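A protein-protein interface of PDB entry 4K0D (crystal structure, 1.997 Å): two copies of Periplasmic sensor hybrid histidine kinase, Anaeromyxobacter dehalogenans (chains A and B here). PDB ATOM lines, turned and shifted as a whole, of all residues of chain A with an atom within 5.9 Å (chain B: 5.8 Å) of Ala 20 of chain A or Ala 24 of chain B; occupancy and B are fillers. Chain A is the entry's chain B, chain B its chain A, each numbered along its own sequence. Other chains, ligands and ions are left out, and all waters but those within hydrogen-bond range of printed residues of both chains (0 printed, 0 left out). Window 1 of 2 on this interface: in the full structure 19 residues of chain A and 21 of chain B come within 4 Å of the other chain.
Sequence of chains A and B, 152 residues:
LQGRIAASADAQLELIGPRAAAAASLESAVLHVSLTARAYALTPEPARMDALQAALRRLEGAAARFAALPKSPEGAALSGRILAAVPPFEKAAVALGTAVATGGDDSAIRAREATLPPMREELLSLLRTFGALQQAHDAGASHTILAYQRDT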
ATOM      1  N   LEU A  15      11.160   5.245 -17.612  1.00  0.00           N
ATOM      2  CA  LEU A  15      11.749   6.461 -17.130  1.00  0.00           C
ATOM      3  C   LEU A  15      12.085   7.449 -18.261  1.00  0.00           C
ATOM      4  O   LEU A  15      12.248   8.636 -18.024  1.00  0.00           O
ATOM      5  CB  LEU A  15      12.991   6.171 -16.313  1.00  0.00           C
ATOM      6  CG  LEU A  15      12.770   5.521 -14.950  1.00  0.00           C
ATOM      7  CD1 LEU A  15      14.103   5.039 -14.440  1.00  0.00           C
ATOM      8  CD2 LEU A  15      12.175   6.503 -13.986  1.00  0.00           C
ATOM      9  N   ILE A  16      12.176   6.974 -19.488  1.00  0.00           N
ATOM     10  CA  ILE A  16      12.604   7.855 -20.583  1.00  0.00           C
ATOM     11  C   ILE A  16      11.739   9.088 -20.687  1.00  0.00           C
ATOM     12  O   ILE A  16      12.232  10.185 -20.673  1.00  0.00           O
ATOM     13  CB  ILE A  16      12.594   7.110 -21.919  1.00  0.00           C
ATOM     14  CG1 ILE A  16      13.860   6.239 -21.995  1.00  0.00           C
ATOM     15  CG2 ILE A  16      12.434   8.108 -23.115  1.00  0.00           C
ATOM     16  CD1 ILE A  16      13.820   5.098 -23.018  1.00  0.00           C
ATOM     17  N   GLY A  17      10.438   8.900 -20.753  1.00  0.00           N
ATOM     18  CA  GLY A  17       9.524   9.980 -21.035  1.00  0.00           C
ATOM     19  C   GLY A  17       9.540  11.050 -19.965  1.00  0.00           C
ATOM     20  O   GLY A  17       9.718  12.209 -20.253  1.00  0.00           O
ATOM     21  N   PRO A  18       9.330  10.663 -18.715  1.00  0.00           N
ATOM     22  CA  PRO A  18       9.318  11.631 -17.612  1.00  0.00           C
ATOM     23  C   PRO A  18      10.625  12.364 -17.465  1.00  0.00           C
ATOM     24  O   PRO A  18      10.623  13.571 -17.151  1.00  0.00           O
ATOM     25  CB  PRO A  18       9.094  10.761 -16.391  1.00  0.00           C
ATOM     26  CG  PRO A  18       8.393   9.546 -16.936  1.00  0.00           C
ATOM     27  CD  PRO A  18       8.824   9.337 -18.319  1.00  0.00           C
ATOM     28  N   ARG A  19      11.733  11.674 -17.691  1.00  0.00           N
ATOM     29  CA  ARG A  19      13.026  12.323 -17.535  1.00  0.00           C
ATOM     30  C   ARG A  19      13.173  13.361 -18.620  1.00  0.00           C
ATOM     31  O   ARG A  19      13.627  14.502 -18.378  1.00  0.00           O
ATOM     32  CB  ARG A  19      14.153  11.306 -17.599  1.00  0.00           C
ATOM     33  CG  ARG A  19      15.554  11.893 -17.429  1.00  0.00           C
ATOM     34  CD  ARG A  19      16.631  10.810 -17.225  1.00  0.00           C
ATOM     35  NE  ARG A  19      16.447   9.667 -18.138  1.00  0.00           N
ATOM     36  CZ  ARG A  19      16.376   8.376 -17.757  1.00  0.00           C
ATOM     37  NH1 ARG A  19      16.470   8.008 -16.473  1.00  0.00           N
ATOM     38  NH2 ARG A  19      16.218   7.432 -18.680  1.00  0.00           N
ATOM     39  N   ALA A  20      12.733  13.013 -19.815  1.00  0.00           N
ATOM     40  CA  ALA A  20      12.880  13.945 -20.925  1.00  0.00           C
ATOM     41  C   ALA A  20      12.003  15.162 -20.664  1.00  0.00           C
ATOM     42  O   ALA A  20      12.346  16.292 -21.034  1.00  0.00           O
ATOM     43  CB  ALA A  20      12.482  13.316 -22.192  1.00  0.00           C
ATOM     44  N   ALA A  21      10.847  14.908 -20.075  1.00  0.00           N
ATOM     45  CA  ALA A  21       9.858  15.937 -19.866  1.00  0.00           C
ATOM     46  C   ALA A  21      10.390  16.901 -18.826  1.00  0.00           C
ATOM     47  O   ALA A  21      10.229  18.103 -18.957  1.00  0.00           O
ATOM     48  CB  ALA A  21       8.503  15.338 -19.429  1.00  0.00           C
ATOM     49  N   ALA A  22      11.031  16.362 -17.801  1.00  0.00           N
ATOM     50  CA  ALA A  22      11.515  17.162 -16.700  1.00  0.00           C
ATOM     51  C   ALA A  22      12.719  18.041 -17.113  1.00  0.00           C
ATOM     52  O   ALA A  22      12.930  19.123 -16.586  1.00  0.00           O
ATOM     53  CB  ALA A  22      11.885  16.253 -15.518  1.00  0.00           C
ATOM     54  N   ALA A  23      13.490  17.556 -18.074  1.00  0.00           N
ATOM     55  CA  ALA A  23      14.563  18.292 -18.664  1.00  0.00           C
ATOM     56  C   ALA A  23      14.009  19.470 -19.503  1.00  0.00           C
ATOM     57  O   ALA A  23      14.460  20.619 -19.345  1.00  0.00           O
ATOM     58  CB  ALA A  23      15.421  17.374 -19.533  1.00  0.00           C
ATOM     59  N   ALA A  24      13.045  19.188 -20.379  1.00  0.00           N
ATOM     60  CA  ALA A  24      12.456  20.264 -21.192  1.00  0.00           C
ATOM     61  C   ALA A  24      11.811  21.293 -20.297  1.00  0.00           C
ATOM     62  O   ALA A  24      11.888  22.508 -20.546  1.00  0.00           O
ATOM     63  CB  ALA A  24      11.437  19.721 -22.174  1.00  0.00           C
ATOM     64  N   SER A  25      11.151  20.815 -19.259  1.00  0.00           N
ATOM     65  CA  SER A  25      10.408  21.695 -18.378  1.00  0.00           C
ATOM     66  C   SER A  25      11.325  22.631 -17.603  1.00  0.00           C
ATOM     67  O   SER A  25      10.961  23.783 -17.354  1.00  0.00           O
ATOM     68  CB  SER A  25       9.614  20.874 -17.384  1.00  0.00           C
ATOM     69  OG  SER A  25       8.254  21.009 -17.701  1.00  0.00           O
ATOM     70  N   LEU A  69      14.641  12.616 -10.508  1.00  0.00           N
ATOM     71  CA  LEU A  69      14.644  11.441 -11.394  1.00  0.00           C
ATOM     72  C   LEU A  69      16.036  10.808 -11.505  1.00  0.00           C
ATOM     73  O   LEU A  69      17.033  11.526 -11.481  1.00  0.00           O
ATOM     74  CB  LEU A  69      14.156  11.834 -12.778  1.00  0.00           C
ATOM     75  CG  LEU A  69      12.702  12.236 -12.806  1.00  0.00           C
ATOM     76  CD1 LEU A  69      12.256  12.930 -14.147  1.00  0.00           C
ATOM     77  CD2 LEU A  69      11.802  11.021 -12.463  1.00  0.00           C
ATOM     78  N   ARG B  19       5.919  20.388 -26.228  1.00  0.00           N
ATOM     79  CA  ARG B  19       6.276  19.787 -27.506  1.00  0.00           C
ATOM     80  C   ARG B  19       7.272  18.660 -27.248  1.00  0.00           C
ATOM     81  O   ARG B  19       7.130  17.552 -27.794  1.00  0.00           O
ATOM     82  CB  ARG B  19       6.894  20.784 -28.462  1.00  0.00           C
ATOM     83  CG  ARG B  19       6.884  20.291 -29.888  1.00  0.00           C
ATOM     84  CD  ARG B  19       7.044  21.456 -30.883  1.00  0.00           C
ATOM     85  NE  ARG B  19       7.880  22.477 -30.288  1.00  0.00           N
ATOM     86  CZ  ARG B  19       7.649  23.785 -30.312  1.00  0.00           C
ATOM     87  NH1 ARG B  19       6.577  24.266 -30.937  1.00  0.00           N
ATOM     88  NH2 ARG B  19       8.518  24.609 -29.714  1.00  0.00           N
ATOM     89  N   ALA B  20       8.231  18.932 -26.365  1.00  0.00           N
ATOM     90  CA  ALA B  20       9.291  17.971 -26.082  1.00  0.00           C
ATOM     91  C   ALA B  20       8.657  16.793 -25.397  1.00  0.00           C
ATOM     92  O   ALA B  20       9.054  15.661 -25.656  1.00  0.00           O
ATOM     93  CB  ALA B  20      10.389  18.551 -25.211  1.00  0.00           C
ATOM     94  N   ALA B  21       7.655  17.066 -24.553  1.00  0.00           N
ATOM     95  CA  ALA B  21       7.005  16.035 -23.762  1.00  0.00           C
ATOM     96  C   ALA B  21       6.223  15.119 -24.683  1.00  0.00           C
ATOM     97  O   ALA B  21       6.213  13.896 -24.501  1.00  0.00           O
ATOM     98  CB  ALA B  21       6.081  16.621 -22.721  1.00  0.00           C
ATOM     99  N   ALA B  22       5.567  15.704 -25.677  1.00  0.00           N
ATOM    100  CA  ALA B  22       4.764  14.894 -26.577  1.00  0.00           C
ATOM    101  C   ALA B  22       5.656  14.037 -27.454  1.00  0.00           C
ATOM    102  O   ALA B  22       5.343  12.878 -27.745  1.00  0.00           O
ATOM    103  CB  ALA B  22       3.847  15.752 -27.439  1.00  0.00           C
ATOM    104  N   ALA B  23       6.752  14.601 -27.912  1.00  0.00           N
ATOM    105  CA  ALA B  23       7.697  13.810 -28.693  1.00  0.00           C
ATOM    106  C   ALA B  23       8.202  12.614 -27.889  1.00  0.00           C
ATOM    107  O   ALA B  23       8.288  11.528 -28.426  1.00  0.00           O
ATOM    108  CB  ALA B  23       8.853  14.676 -29.124  1.00  0.00           C
ATOM    109  N   ALA B  24       8.554  12.812 -26.617  1.00  0.00           N
ATOM    110  CA  ALA B  24       9.122  11.720 -25.841  1.00  0.00           C
ATOM    111  C   ALA B  24       8.101  10.697 -25.513  1.00  0.00           C
ATOM    112  O   ALA B  24       8.427   9.540 -25.391  1.00  0.00           O
ATOM    113  CB  ALA B  24       9.759  12.149 -24.601  1.00  0.00           C
ATOM    114  N   SER B  25       6.856  11.121 -25.358  1.00  0.00           N
ATOM    115  CA  SER B  25       5.779  10.204 -25.061  1.00  0.00           C
ATOM    116  C   SER B  25       5.390   9.380 -26.273  1.00  0.00           C
ATOM    117  O   SER B  25       4.986   8.244 -26.139  1.00  0.00           O
ATOM    118  CB  SER B  25       4.579  10.933 -24.466  1.00  0.00           C
ATOM    119  OG  SER B  25       4.851  11.241 -23.115  1.00  0.00           O
ATOM    120  N   LEU B  26       5.532   9.938 -27.462  1.00  0.00           N
ATOM    121  CA  LEU B  26       5.340   9.134 -28.633  1.00  0.00           C
ATOM    122  C   LEU B  26       6.518   8.110 -28.765  1.00  0.00           C
ATOM    123  O   LEU B  26       6.316   6.928 -29.040  1.00  0.00           O
ATOM    124  CB  LEU B  26       5.211  10.013 -29.851  1.00  0.00           C
ATOM    125  CG  LEU B  26       5.081   9.202 -31.117  1.00  0.00           C
ATOM    126  CD1 LEU B  26       3.980   8.196 -31.010  1.00  0.00           C
ATOM    127  CD2 LEU B  26       4.788  10.089 -32.274  1.00  0.00           C
ATOM    128  N   GLU B  27       7.716   8.572 -28.516  1.00  0.00           N
ATOM    129  CA  GLU B  27       8.838   7.730 -28.458  1.00  0.00           C
ATOM    130  C   GLU B  27       8.576   6.564 -27.517  1.00  0.00           C
ATOM    131  O   GLU B  27       8.764   5.457 -27.881  1.00  0.00           O
ATOM    132  CB  GLU B  27      10.062   8.517 -28.052  1.00  0.00           C
ATOM    133  CG  GLU B  27      10.986   8.737 -29.223  1.00  0.00           C
ATOM    134  CD  GLU B  27      11.778  10.030 -29.231  1.00  0.00           C
ATOM    135  OE1 GLU B  27      12.436  10.376 -28.267  1.00  0.00           O
ATOM    136  OE2 GLU B  27      11.778  10.699 -30.262  1.00  0.00           O
ATOM    137  N   SER B  28       8.127   6.861 -26.324  1.00  0.00           N
ATOM    138  CA  SER B  28       8.019   5.869 -25.265  1.00  0.00           C
ATOM    139  C   SER B  28       6.853   4.892 -25.621  1.00  0.00           C
ATOM    140  O   SER B  28       6.933   3.670 -25.389  1.00  0.00           O
ATOM    141  CB  SER B  28       7.818   6.633 -23.954  1.00  0.00           C
ATOM    142  OG  SER B  28       7.717   5.829 -22.812  1.00  0.00           O
ATOM    143  N   ALA B  29       5.813   5.412 -26.262  1.00  0.00           N
ATOM    144  CA  ALA B  29       4.702   4.568 -26.696  1.00  0.00           C
ATOM    145  C   ALA B  29       5.193   3.567 -27.750  1.00  0.00           C
ATOM    146  O   ALA B  29       4.717   2.441 -27.814  1.00  0.00           O
ATOM    147  CB  ALA B  29       3.504   5.438 -27.267  1.00  0.00           C
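Among the printed residues, pairs that only touch across the chains: Ala 20 of chain A with Ala 24 of chain B (3.8 Å) and Ala 24 of chain A with Ala 20 of chain B (3.4 Å).
Of the 12 printed residues of chain A, 2 touch a printed residue of chain B.
Hydrophobic or aromatic side chains of chain A that line the printed part of chain B: Ala 20 and Ala 24.
Ala 20 of chain A touches Ala 24 of chain B, and with the chains exchanged Ala 24 of chain A touches Ala 20 of chain B.
Positions printed for both chains: 19, 20, 21, 22, 23, 24 and 25.
Ala 20 of chain A touches just one residue of chain B: Ala 24.
Of the printed residues of chain A, Ala 20 of chain B touches Ala 24 (3.4 Å).
Of the printed residues of chain B, Ala 24 of chain A touches Ala 20 (3.4 Å).
Ala 21 of chain A touches none of the printed residues of chain B.
Leu 69 of chain A touches none of the printed residues of chain B.
The nearest residue of chain A that does not touch Ala 24 of chain B is Gly 17 of chain A (4.2 Å).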
